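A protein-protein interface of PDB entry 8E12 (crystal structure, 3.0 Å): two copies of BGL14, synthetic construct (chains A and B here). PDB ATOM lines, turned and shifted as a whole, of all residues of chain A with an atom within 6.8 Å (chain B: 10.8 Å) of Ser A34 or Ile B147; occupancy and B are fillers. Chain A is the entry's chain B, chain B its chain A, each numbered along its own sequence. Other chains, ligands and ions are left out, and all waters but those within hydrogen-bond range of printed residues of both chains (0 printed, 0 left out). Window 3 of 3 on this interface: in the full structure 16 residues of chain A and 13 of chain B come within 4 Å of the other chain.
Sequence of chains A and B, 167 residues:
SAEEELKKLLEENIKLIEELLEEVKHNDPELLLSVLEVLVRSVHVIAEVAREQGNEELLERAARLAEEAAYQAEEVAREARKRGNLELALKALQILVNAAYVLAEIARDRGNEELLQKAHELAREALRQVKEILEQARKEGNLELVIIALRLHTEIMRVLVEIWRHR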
ATOM      1  N   LEU A  20       8.197  -4.974   8.358  1.00  0.00           N
ATOM      2  CA  LEU A  20       9.160  -5.059   7.265  1.00  0.00           C
ATOM      3  C   LEU A  20       8.659  -5.984   6.163  1.00  0.00           C
ATOM      4  O   LEU A  20       8.852  -5.702   4.975  1.00  0.00           O
ATOM      5  CB  LEU A  20      10.512  -5.534   7.794  1.00  0.00           C
ATOM      6  CG  LEU A  20      11.671  -5.464   6.800  1.00  0.00           C
ATOM      7  CD1 LEU A  20      11.971  -4.019   6.439  1.00  0.00           C
ATOM      8  CD2 LEU A  20      12.900  -6.149   7.369  1.00  0.00           C
ATOM      9  N   VAL A  24       8.458  -4.894   2.460  1.00  0.00           N
ATOM     10  CA  VAL A  24       9.323  -5.513   1.462  1.00  0.00           C
ATOM     11  C   VAL A  24       8.532  -6.371   0.485  1.00  0.00           C
ATOM     12  O   VAL A  24       9.111  -6.888  -0.485  1.00  0.00           O
ATOM     13  CB  VAL A  24      10.406  -6.370   2.147  1.00  0.00           C
ATOM     14  CG1 VAL A  24       9.813  -7.698   2.577  1.00  0.00           C
ATOM     15  CG2 VAL A  24      11.620  -6.560   1.243  1.00  0.00           C
ATOM     16  N   PRO A  29      12.244  -9.834  -4.945  1.00  0.00           N
ATOM     17  CA  PRO A  29      12.073 -11.152  -4.307  1.00  0.00           C
ATOM     18  C   PRO A  29      13.256 -11.577  -3.451  1.00  0.00           C
ATOM     19  O   PRO A  29      13.062 -12.233  -2.420  1.00  0.00           O
ATOM     20  CB  PRO A  29      11.871 -12.092  -5.505  1.00  0.00           C
ATOM     21  CG  PRO A  29      11.344 -11.215  -6.585  1.00  0.00           C
ATOM     22  CD  PRO A  29      12.010  -9.885  -6.398  1.00  0.00           C
ATOM     23  N   GLU A  30      14.481 -11.241  -3.866  1.00  0.00           N
ATOM     24  CA  GLU A  30      15.651 -11.567  -3.058  1.00  0.00           C
ATOM     25  C   GLU A  30      15.576 -10.902  -1.690  1.00  0.00           C
ATOM     26  O   GLU A  30      15.911 -11.517  -0.671  1.00  0.00           O
ATOM     27  CB  GLU A  30      16.927 -11.152  -3.793  1.00  0.00           C
ATOM     28  N   LEU A  31      15.151  -9.636  -1.647  1.00  0.00           N
ATOM     29  CA  LEU A  31      14.949  -8.967  -0.366  1.00  0.00           C
ATOM     30  C   LEU A  31      13.813  -9.611   0.419  1.00  0.00           C
ATOM     31  O   LEU A  31      13.885  -9.718   1.649  1.00  0.00           O
ATOM     32  CB  LEU A  31      14.679  -7.479  -0.587  1.00  0.00           C
ATOM     33  CG  LEU A  31      15.591  -6.512   0.170  1.00  0.00           C
ATOM     34  N   LEU A  32      12.753 -10.039  -0.274  1.00  0.00           N
ATOM     35  CA  LEU A  32      11.652 -10.728   0.394  1.00  0.00           C
ATOM     36  C   LEU A  32      12.119 -12.033   1.022  1.00  0.00           C
ATOM     37  O   LEU A  32      11.677 -12.396   2.119  1.00  0.00           O
ATOM     38  CB  LEU A  32      10.515 -10.991  -0.591  1.00  0.00           C
ATOM     39  CG  LEU A  32       9.213 -11.508   0.023  1.00  0.00           C
ATOM     40  CD1 LEU A  32       8.420 -10.381   0.659  1.00  0.00           C
ATOM     41  CD2 LEU A  32       8.374 -12.225  -1.018  1.00  0.00           C
ATOM     42  N   LEU A  33      13.005 -12.758   0.336  1.00  0.00           N
ATOM     43  CA  LEU A  33      13.550 -13.988   0.900  1.00  0.00           C
ATOM     44  C   LEU A  33      14.359 -13.702   2.157  1.00  0.00           C
ATOM     45  O   LEU A  33      14.385 -14.522   3.082  1.00  0.00           O
ATOM     46  CB  LEU A  33      14.405 -14.710  -0.140  1.00  0.00           C
ATOM     47  CG  LEU A  33      13.658 -15.532  -1.195  1.00  0.00           C
ATOM     48  CD1 LEU A  33      14.555 -16.622  -1.756  1.00  0.00           C
ATOM     49  CD2 LEU A  33      12.367 -16.125  -0.640  1.00  0.00           C
ATOM     50  N   SER A  34      15.027 -12.546   2.208  1.00  0.00           N
ATOM     51  CA  SER A  34      15.818 -12.198   3.382  1.00  0.00           C
ATOM     52  C   SER A  34      14.929 -12.012   4.604  1.00  0.00           C
ATOM     53  O   SER A  34      15.272 -12.461   5.704  1.00  0.00           O
ATOM     54  CB  SER A  34      16.635 -10.934   3.110  1.00  0.00           C
ATOM     55  OG  SER A  34      17.913 -11.254   2.589  1.00  0.00           O
ATOM     56  N   VAL A  35      13.784 -11.343   4.435  1.00  0.00           N
ATOM     57  CA  VAL A  35      12.861 -11.165   5.551  1.00  0.00           C
ATOM     58  C   VAL A  35      12.289 -12.507   5.990  1.00  0.00           C
ATOM     59  O   VAL A  35      12.146 -12.774   7.189  1.00  0.00           O
ATOM     60  CB  VAL A  35      11.738 -10.185   5.166  1.00  0.00           C
ATOM     61  CG1 VAL A  35      10.835  -9.906   6.362  1.00  0.00           C
ATOM     62  CG2 VAL A  35      12.313  -8.905   4.610  1.00  0.00           C
ATOM     63  N   LEU A  36      11.952 -13.371   5.029  1.00  0.00           N
ATOM     64  CA  LEU A  36      11.466 -14.703   5.370  1.00  0.00           C
ATOM     65  C   LEU A  36      12.530 -15.529   6.077  1.00  0.00           C
ATOM     66  O   LEU A  36      12.205 -16.348   6.943  1.00  0.00           O
ATOM     67  CB  LEU A  36      10.975 -15.423   4.114  1.00  0.00           C
ATOM     68  CG  LEU A  36       9.851 -14.719   3.355  1.00  0.00           C
ATOM     69  CD1 LEU A  36       9.746 -15.245   1.930  1.00  0.00           C
ATOM     70  CD2 LEU A  36       8.532 -14.867   4.095  1.00  0.00           C
ATOM     71  N   GLU A  37      13.801 -15.340   5.716  1.00  0.00           N
ATOM     72  CA  GLU A  37      14.879 -16.042   6.405  1.00  0.00           C
ATOM     73  C   GLU A  37      14.949 -15.651   7.876  1.00  0.00           C
ATOM     74  O   GLU A  37      15.122 -16.510   8.747  1.00  0.00           O
ATOM     75  CB  GLU A  37      16.209 -15.758   5.710  1.00  0.00           C
ATOM     76  CG  GLU A  37      17.216 -16.888   5.810  1.00  0.00           C
ATOM     77  CD  GLU A  37      18.644 -16.387   5.817  1.00  0.00           C
ATOM     78  OE1 GLU A  37      19.348 -16.603   6.826  1.00  0.00           O
ATOM     79  OE2 GLU A  37      19.063 -15.775   4.811  1.00  0.00           O
ATOM     80  N   VAL A  38      14.822 -14.356   8.172  1.00  0.00           N
ATOM     81  CA  VAL A  38      14.824 -13.907   9.559  1.00  0.00           C
ATOM     82  C   VAL A  38      13.540 -14.330  10.264  1.00  0.00           C
ATOM     83  O   VAL A  38      13.549 -14.661  11.456  1.00  0.00           O
ATOM     84  CB  VAL A  38      15.034 -12.381   9.619  1.00  0.00           C
ATOM     85  CG1 VAL A  38      14.874 -11.862  11.043  1.00  0.00           C
ATOM     86  CG2 VAL A  38      16.399 -12.011   9.056  1.00  0.00           C
ATOM     87  N   LEU A  39      12.417 -14.331   9.539  1.00  0.00           N
ATOM     88  CA  LEU A  39      11.138 -14.702  10.138  1.00  0.00           C
ATOM     89  C   LEU A  39      11.159 -16.136  10.660  1.00  0.00           C
ATOM     90  O   LEU A  39      10.827 -16.387  11.824  1.00  0.00           O
ATOM     91  CB  LEU A  39      10.011 -14.513   9.120  1.00  0.00           C
ATOM     92  CG  LEU A  39       8.608 -14.946   9.550  1.00  0.00           C
ATOM     93  CD1 LEU A  39       8.265 -14.382  10.924  1.00  0.00           C
ATOM     94  CD2 LEU A  39       7.570 -14.529   8.520  1.00  0.00           C
ATOM     95  N   ILE A  95      14.122 -21.724   2.264  1.00  0.00           N
ATOM     96  CA  ILE A  95      13.302 -21.074   3.278  1.00  0.00           C
ATOM     97  C   ILE A  95      11.977 -21.809   3.452  1.00  0.00           C
ATOM     98  O   ILE A  95      11.403 -21.821   4.548  1.00  0.00           O
ATOM     99  CB  ILE A  95      13.096 -19.596   2.906  1.00  0.00           C
ATOM    100  CG1 ILE A  95      14.453 -18.924   2.698  1.00  0.00           C
ATOM    101  CG2 ILE A  95      12.308 -18.871   3.985  1.00  0.00           C
ATOM    102  CD1 ILE A  95      14.366 -17.546   2.111  1.00  0.00           C
ATOM    103  N   LEU B  86      28.164   0.776   9.349  1.00  0.00           N
ATOM    104  CA  LEU B  86      27.136   0.069  10.105  1.00  0.00           C
ATOM    105  C   LEU B  86      27.240  -1.439   9.927  1.00  0.00           C
ATOM    106  O   LEU B  86      26.834  -2.196  10.816  1.00  0.00           O
ATOM    107  CB  LEU B  86      25.749   0.563   9.696  1.00  0.00           C
ATOM    108  CG  LEU B  86      25.158   1.757  10.453  1.00  0.00           C
ATOM    109  CD1 LEU B  86      26.186   2.856  10.687  1.00  0.00           C
ATOM    110  CD2 LEU B  86      23.953   2.311   9.708  1.00  0.00           C
ATOM    111  N   GLU B  87      27.775  -1.895   8.791  1.00  0.00           N
ATOM    112  CA  GLU B  87      27.910  -3.329   8.562  1.00  0.00           C
ATOM    113  C   GLU B  87      28.911  -3.938   9.533  1.00  0.00           C
ATOM    114  O   GLU B  87      28.611  -4.925  10.216  1.00  0.00           O
ATOM    115  CB  GLU B  87      28.320  -3.602   7.116  1.00  0.00           C
ATOM    116  CG  GLU B  87      27.245  -4.305   6.303  1.00  0.00           C
ATOM    117  CD  GLU B  87      27.811  -5.111   5.148  1.00  0.00           C
ATOM    118  OE1 GLU B  87      27.818  -6.357   5.242  1.00  0.00           O
ATOM    119  OE2 GLU B  87      28.241  -4.500   4.147  1.00  0.00           O
ATOM    120  N   LEU B  90      27.342  -3.859  12.970  1.00  0.00           N
ATOM    121  CA  LEU B  90      26.372  -4.935  13.149  1.00  0.00           C
ATOM    122  C   LEU B  90      27.060  -6.294  13.187  1.00  0.00           C
ATOM    123  O   LEU B  90      26.654  -7.183  13.945  1.00  0.00           O
ATOM    124  CB  LEU B  90      25.328  -4.892  12.034  1.00  0.00           C
ATOM    125  CG  LEU B  90      24.118  -3.997  12.301  1.00  0.00           C
ATOM    126  CD1 LEU B  90      23.357  -3.707  11.015  1.00  0.00           C
ATOM    127  CD2 LEU B  90      23.209  -4.630  13.342  1.00  0.00           C
ATOM    128  N   LYS B  91      28.107  -6.471  12.377  1.00  0.00           N
ATOM    129  CA  LYS B  91      28.883  -7.705  12.427  1.00  0.00           C
ATOM    130  C   LYS B  91      29.541  -7.888  13.788  1.00  0.00           C
ATOM    131  O   LYS B  91      29.533  -8.990  14.343  1.00  0.00           O
ATOM    132  CB  LYS B  91      29.935  -7.706  11.317  1.00  0.00           C
ATOM    133  CG  LYS B  91      30.623  -9.044  11.108  1.00  0.00           C
ATOM    134  CD  LYS B  91      31.409  -9.062   9.806  1.00  0.00           C
ATOM    135  N   GLN B  94      27.322  -9.140  16.605  1.00  0.00           N
ATOM    136  CA  GLN B  94      27.032 -10.571  16.578  1.00  0.00           C
ATOM    137  C   GLN B  94      27.960 -11.344  17.509  1.00  0.00           C
ATOM    138  O   GLN B  94      27.510 -12.186  18.292  1.00  0.00           O
ATOM    139  CB  GLN B  94      27.135 -11.101  15.149  1.00  0.00           C
ATOM    140  CG  GLN B  94      26.305 -12.348  14.894  1.00  0.00           C
ATOM    141  N   VAL B 130      21.826  -2.004  18.284  1.00  0.00           N
ATOM    142  CA  VAL B 130      21.042  -2.372  17.107  1.00  0.00           C
ATOM    143  C   VAL B 130      19.811  -1.481  16.991  1.00  0.00           C
ATOM    144  O   VAL B 130      19.409  -1.095  15.888  1.00  0.00           O
ATOM    145  CB  VAL B 130      20.662  -3.867  17.145  1.00  0.00           C
ATOM    146  CG1 VAL B 130      20.032  -4.238  18.471  1.00  0.00           C
ATOM    147  CG2 VAL B 130      19.729  -4.217  15.992  1.00  0.00           C
ATOM    148  N   ILE B 133      21.136   1.581  15.528  1.00  0.00           N
ATOM    149  CA  ILE B 133      21.461   1.299  14.135  1.00  0.00           C
ATOM    150  C   ILE B 133      20.190   1.124  13.312  1.00  0.00           C
ATOM    151  O   ILE B 133      20.113   1.565  12.159  1.00  0.00           O
ATOM    152  CB  ILE B 133      22.375   0.062  14.048  1.00  0.00           C
ATOM    153  CG1 ILE B 133      23.798   0.422  14.481  1.00  0.00           C
ATOM    154  CG2 ILE B 133      22.381  -0.521  12.642  1.00  0.00           C
ATOM    155  CD1 ILE B 133      24.700  -0.776  14.677  1.00  0.00           C
ATOM    156  N   LEU B 134      19.169   0.489  13.895  1.00  0.00           N
ATOM    157  CA  LEU B 134      17.932   0.227  13.164  1.00  0.00           C
ATOM    158  C   LEU B 134      17.257   1.522  12.736  1.00  0.00           C
ATOM    159  O   LEU B 134      16.880   1.683  11.568  1.00  0.00           O
ATOM    160  CB  LEU B 134      16.986  -0.604  14.030  1.00  0.00           C
ATOM    161  CG  LEU B 134      16.789  -2.069  13.650  1.00  0.00           C
ATOM    162  CD1 LEU B 134      15.925  -2.765  14.686  1.00  0.00           C
ATOM    163  CD2 LEU B 134      16.176  -2.180  12.264  1.00  0.00           C
ATOM    164  N   GLU B 135      17.084   2.459  13.672  1.00  0.00           N
ATOM    165  CA  GLU B 135      16.470   3.736  13.324  1.00  0.00           C
ATOM    166  C   GLU B 135      17.338   4.507  12.336  1.00  0.00           C
ATOM    167  O   GLU B 135      16.818   5.208  11.460  1.00  0.00           O
ATOM    168  CB  GLU B 135      16.193   4.558  14.588  1.00  0.00           C
ATOM    169  CG  GLU B 135      17.198   5.662  14.892  1.00  0.00           C
ATOM    170  CD  GLU B 135      16.797   6.505  16.088  1.00  0.00           C
ATOM    171  OE1 GLU B 135      17.628   7.314  16.553  1.00  0.00           O
ATOM    172  OE2 GLU B 135      15.651   6.361  16.563  1.00  0.00           O
ATOM    173  N   GLN B 136      18.663   4.391  12.461  1.00  0.00           N
ATOM    174  CA  GLN B 136      19.550   5.028  11.494  1.00  0.00           C
ATOM    175  C   GLN B 136      19.449   4.352  10.132  1.00  0.00           C
ATOM    176  O   GLN B 136      19.349   5.026   9.101  1.00  0.00           O
ATOM    177  CB  GLN B 136      20.990   5.000  12.006  1.00  0.00           C
ATOM    178  N   ALA B 137      19.466   3.016  10.108  1.00  0.00           N
ATOM    179  CA  ALA B 137      19.368   2.300   8.839  1.00  0.00           C
ATOM    180  C   ALA B 137      18.038   2.579   8.151  1.00  0.00           C
ATOM    181  O   ALA B 137      17.986   2.748   6.927  1.00  0.00           O
ATOM    182  CB  ALA B 137      19.555   0.799   9.063  1.00  0.00           C
ATOM    183  N   ARG B 138      16.953   2.636   8.926  1.00  0.00           N
ATOM    184  CA  ARG B 138      15.650   2.972   8.362  1.00  0.00           C
ATOM    185  C   ARG B 138      15.632   4.394   7.813  1.00  0.00           C
ATOM    186  O   ARG B 138      14.974   4.666   6.801  1.00  0.00           O
ATOM    187  CB  ARG B 138      14.561   2.790   9.418  1.00  0.00           C
ATOM    188  N   GLY B 141      17.260   4.639   4.431  1.00  0.00           N
ATOM    189  CA  GLY B 141      16.595   3.856   3.412  1.00  0.00           C
ATOM    190  C   GLY B 141      17.270   2.547   3.075  1.00  0.00           C
ATOM    191  O   GLY B 141      16.897   1.914   2.081  1.00  0.00           O
ATOM    192  N   ASN B 142      18.255   2.121   3.864  1.00  0.00           N
ATOM    193  CA  ASN B 142      18.982   0.881   3.606  1.00  0.00           C
ATOM    194  C   ASN B 142      18.203  -0.269   4.232  1.00  0.00           C
ATOM    195  O   ASN B 142      18.419  -0.646   5.384  1.00  0.00           O
ATOM    196  CB  ASN B 142      20.402   0.970   4.155  1.00  0.00           C
ATOM    197  CG  ASN B 142      21.276  -0.194   3.718  1.00  0.00           C
ATOM    198  OD1 ASN B 142      20.843  -1.345   3.698  1.00  0.00           O
ATOM    199  ND2 ASN B 142      22.521   0.107   3.367  1.00  0.00           N
ATOM    200  N   LEU B 143      17.276  -0.832   3.451  1.00  0.00           N
ATOM    201  CA  LEU B 143      16.486  -1.964   3.921  1.00  0.00           C
ATOM    202  C   LEU B 143      17.353  -3.196   4.149  1.00  0.00           C
ATOM    203  O   LEU B 143      16.986  -4.073   4.938  1.00  0.00           O
ATOM    204  CB  LEU B 143      15.369  -2.276   2.926  1.00  0.00           C
ATOM    205  N   GLU B 144      18.485  -3.295   3.450  1.00  0.00           N
ATOM    206  CA  GLU B 144      19.385  -4.424   3.654  1.00  0.00           C
ATOM    207  C   GLU B 144      19.959  -4.427   5.066  1.00  0.00           C
ATOM    208  O   GLU B 144      20.094  -5.487   5.688  1.00  0.00           O
ATOM    209  CB  GLU B 144      20.509  -4.389   2.621  1.00  0.00           C
ATOM    210  CG  GLU B 144      20.095  -4.855   1.238  1.00  0.00           C
ATOM    211  CD  GLU B 144      20.852  -4.137   0.141  1.00  0.00           C
ATOM    212  OE1 GLU B 144      20.204  -3.482  -0.703  1.00  0.00           O
ATOM    213  OE2 GLU B 144      22.098  -4.229   0.121  1.00  0.00           O
ATOM    214  N   LEU B 145      20.316  -3.248   5.584  1.00  0.00           N
ATOM    215  CA  LEU B 145      20.901  -3.167   6.919  1.00  0.00           C
ATOM    216  C   LEU B 145      19.892  -3.474   8.017  1.00  0.00           C
ATOM    217  O   LEU B 145      20.272  -3.995   9.071  1.00  0.00           O
ATOM    218  CB  LEU B 145      21.512  -1.784   7.137  1.00  0.00           C
ATOM    219  CG  LEU B 145      23.024  -1.681   6.942  1.00  0.00           C
ATOM    220  CD1 LEU B 145      23.445  -2.247   5.598  1.00  0.00           C
ATOM    221  CD2 LEU B 145      23.454  -0.233   7.065  1.00  0.00           C
ATOM    222  N   VAL B 146      18.613  -3.149   7.809  1.00  0.00           N
ATOM    223  CA  VAL B 146      17.619  -3.496   8.820  1.00  0.00           C
ATOM    224  C   VAL B 146      17.463  -5.010   8.902  1.00  0.00           C
ATOM    225  O   VAL B 146      17.155  -5.552   9.971  1.00  0.00           O
ATOM    226  CB  VAL B 146      16.277  -2.778   8.559  1.00  0.00           C
ATOM    227  CG1 VAL B 146      16.487  -1.270   8.467  1.00  0.00           C
ATOM    228  CG2 VAL B 146      15.579  -3.316   7.325  1.00  0.00           C
ATOM    229  N   ILE B 147      17.672  -5.715   7.784  1.00  0.00           N
ATOM    230  CA  ILE B 147      17.621  -7.176   7.792  1.00  0.00           C
ATOM    231  C   ILE B 147      18.676  -7.738   8.735  1.00  0.00           C
ATOM    232  O   ILE B 147      18.388  -8.584   9.590  1.00  0.00           O
ATOM    233  CB  ILE B 147      17.815  -7.722   6.367  1.00  0.00           C
ATOM    234  CG1 ILE B 147      16.685  -7.256   5.456  1.00  0.00           C
ATOM    235  CG2 ILE B 147      17.916  -9.244   6.389  1.00  0.00           C
ATOM    236  CD1 ILE B 147      15.517  -8.173   5.454  1.00  0.00           C
ATOM    237  N   ILE B 148      19.920  -7.280   8.579  1.00  0.00           N
ATOM    238  CA  ILE B 148      20.995  -7.716   9.464  1.00  0.00           C
ATOM    239  C   ILE B 148      20.691  -7.315  10.899  1.00  0.00           C
ATOM    240  O   ILE B 148      20.918  -8.086  11.840  1.00  0.00           O
ATOM    241  CB  ILE B 148      22.344  -7.147   8.988  1.00  0.00           C
ATOM    242  CG1 ILE B 148      22.462  -7.264   7.465  1.00  0.00           C
ATOM    243  CG2 ILE B 148      23.495  -7.862   9.679  1.00  0.00           C
ATOM    244  CD1 ILE B 148      23.851  -6.980   6.934  1.00  0.00           C
ATOM    245  N   ALA B 149      20.175  -6.098  11.090  1.00  0.00           N
ATOM    246  CA  ALA B 149      19.821  -5.644  12.428  1.00  0.00           C
ATOM    247  C   ALA B 149      18.691  -6.479  13.017  1.00  0.00           C
ATOM    248  O   ALA B 149      18.750  -6.873  14.188  1.00  0.00           O
ATOM    249  CB  ALA B 149      19.435  -4.166  12.388  1.00  0.00           C
ATOM    250  N   LEU B 150      17.665  -6.782  12.219  1.00  0.00           N
ATOM    251  CA  LEU B 150      16.589  -7.636  12.710  1.00  0.00           C
ATOM    252  C   LEU B 150      17.082  -9.055  12.950  1.00  0.00           C
ATOM    253  O   LEU B 150      16.648  -9.716  13.901  1.00  0.00           O
ATOM    254  CB  LEU B 150      15.416  -7.634  11.729  1.00  0.00           C
ATOM    255  CG  LEU B 150      14.538  -6.382  11.670  1.00  0.00           C
ATOM    256  CD1 LEU B 150      13.133  -6.736  11.213  1.00  0.00           C
ATOM    257  CD2 LEU B 150      14.495  -5.684  13.020  1.00  0.00           C
ATOM    258  N   ARG B 151      17.987  -9.543  12.098  1.00  0.00           N
ATOM    259  CA  ARG B 151      18.619 -10.832  12.357  1.00  0.00           C
ATOM    260  C   ARG B 151      19.375 -10.813  13.678  1.00  0.00           C
ATOM    261  O   ARG B 151      19.271 -11.754  14.475  1.00  0.00           O
ATOM    262  CB  ARG B 151      19.552 -11.203  11.205  1.00  0.00           C
ATOM    263  CG  ARG B 151      19.661 -12.698  10.953  1.00  0.00           C
ATOM    264  N   LEU B 152      20.135  -9.745  13.933  1.00  0.00           N
ATOM    265  CA  LEU B 152      20.802  -9.603  15.223  1.00  0.00           C
ATOM    266  C   LEU B 152      19.785  -9.429  16.344  1.00  0.00           C
ATOM    267  O   LEU B 152      19.906 -10.047  17.409  1.00  0.00           O
ATOM    268  CB  LEU B 152      21.775  -8.424  15.186  1.00  0.00           C
ATOM    269  CG  LEU B 152      22.981  -8.511  16.123  1.00  0.00           C
ATOM    270  N   HIS B 153      18.790  -8.563  16.126  1.00  0.00           N
ATOM    271  CA  HIS B 153      17.759  -8.316  17.131  1.00  0.00           C
ATOM    272  C   HIS B 153      17.104  -9.617  17.580  1.00  0.00           C
ATOM    273  O   HIS B 153      16.848  -9.816  18.774  1.00  0.00           O
ATOM    274  CB  HIS B 153      16.724  -7.335  16.567  1.00  0.00           C
ATOM    275  CG  HIS B 153      15.603  -7.008  17.505  1.00  0.00           C
ATOM    276  ND1 HIS B 153      14.680  -7.942  17.923  1.00  0.00           N
ATOM    277  CD2 HIS B 153      15.252  -5.841  18.096  1.00  0.00           C
ATOM    278  CE1 HIS B 153      13.811  -7.367  18.735  1.00  0.00           C
ATOM    279  NE2 HIS B 153      14.135  -6.092  18.857  1.00  0.00           N
ATOM    280  N   THR B 154      16.822 -10.515  16.632  1.00  0.00           N
ATOM    281  CA  THR B 154      16.246 -11.811  16.973  1.00  0.00           C
ATOM    282  C   THR B 154      17.192 -12.633  17.842  1.00  0.00           C
ATOM    283  O   THR B 154      16.757 -13.320  18.773  1.00  0.00           O
ATOM    284  CB  THR B 154      15.900 -12.578  15.698  1.00  0.00           C
ATOM    285  OG1 THR B 154      15.027 -11.788  14.882  1.00  0.00           O
ATOM    286  CG2 THR B 154      15.227 -13.889  16.040  1.00  0.00           C
ATOM    287  N   GLU B 155      18.494 -12.572  17.552  1.00  0.00           N
ATOM    288  CA  GLU B 155      19.458 -13.386  18.284  1.00  0.00           C
ATOM    289  C   GLU B 155      19.576 -12.936  19.735  1.00  0.00           C
ATOM    290  O   GLU B 155      19.815 -13.762  20.623  1.00  0.00           O
ATOM    291  CB  GLU B 155      20.819 -13.340  17.593  1.00  0.00           C
ATOM    292  CG  GLU B 155      21.382 -14.712  17.260  1.00  0.00           C
ATOM    293  CD  GLU B 155      20.413 -15.558  16.458  1.00  0.00           C
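No position is printed for both chains.
Of the 9 pairs that touch across the chains among the printed residues, none has its exchanged pair printed and touching as well.
Of chain B, only Ile B147 (3.8 Å) comes within 4 Å of Ser A34.
Printed residues of chain A within 4 Å of Ile B147: Leu A20, Ser A34, Val A35 and Val A38.
No residue of chain B comes within 4 Å of Glu A30.
No residue of chain B comes within 4 Å of Leu A31.
Of chain B, only Ile B147 (3.4 Å) comes within 4 Å of Val A35.
No residue of chain B comes within 4 Å of Glu A37.
Printed residues of chain A within 4 Å of Thr B154: Val A38.
Of the printed residues of chain A, Val B146 touches Leu A20.
Of the printed residues of chain B, Leu A20 touches Val B146 (3.8 Å), Ile B147 (3.8 Å) and Leu B150 (3.9 Å).
Of the printed residues of chain A, Arg B151 touches Val A38.
Leu A39 touches none of the printed residues of chain B.
Arg B138 touches none of the printed residues of chain A.
The nearest residue of chain B that does not touch Ser A34 is Arg B151 (6.8 Å).
Among the printed residues, pairs that only touch across the chains: Leu A20 with Val B146 (3.8 Å), Leu A20 with Ile B147 (3.8 Å), Leu A20 with Leu B150 (3.9 Å), Ser A34 with Ile B147 (3.8 Å), Val A35 with Ile B147 (3.4 Å), Val A38 with Ile B147 (3.998 Å), Val A38 with Leu B150 (3.99 Å), Val A38 with Arg B151 (3.8 Å) and Val A38 with Thr B154 (3.8 Å).
Printed residues of chain B that touch a printed residue of chain A: Val B146, Ile B147, Leu B150, Arg B151 and Thr B154.
Hydrophobic or aromatic side chains of chain B within 4 Å of the printed part of chain A: Val B146, Ile B147 and Leu B150.
Among the printed residues, no Asp or Glu carboxylate lies within 4 Å of a Lys or Arg side-chain nitrogen of the other chain.
The backbone carbonyl oxygen of Leu B150 is in hydrogen-bond range of the side-chain hydroxyl of Thr B154, at 2.8 Å.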
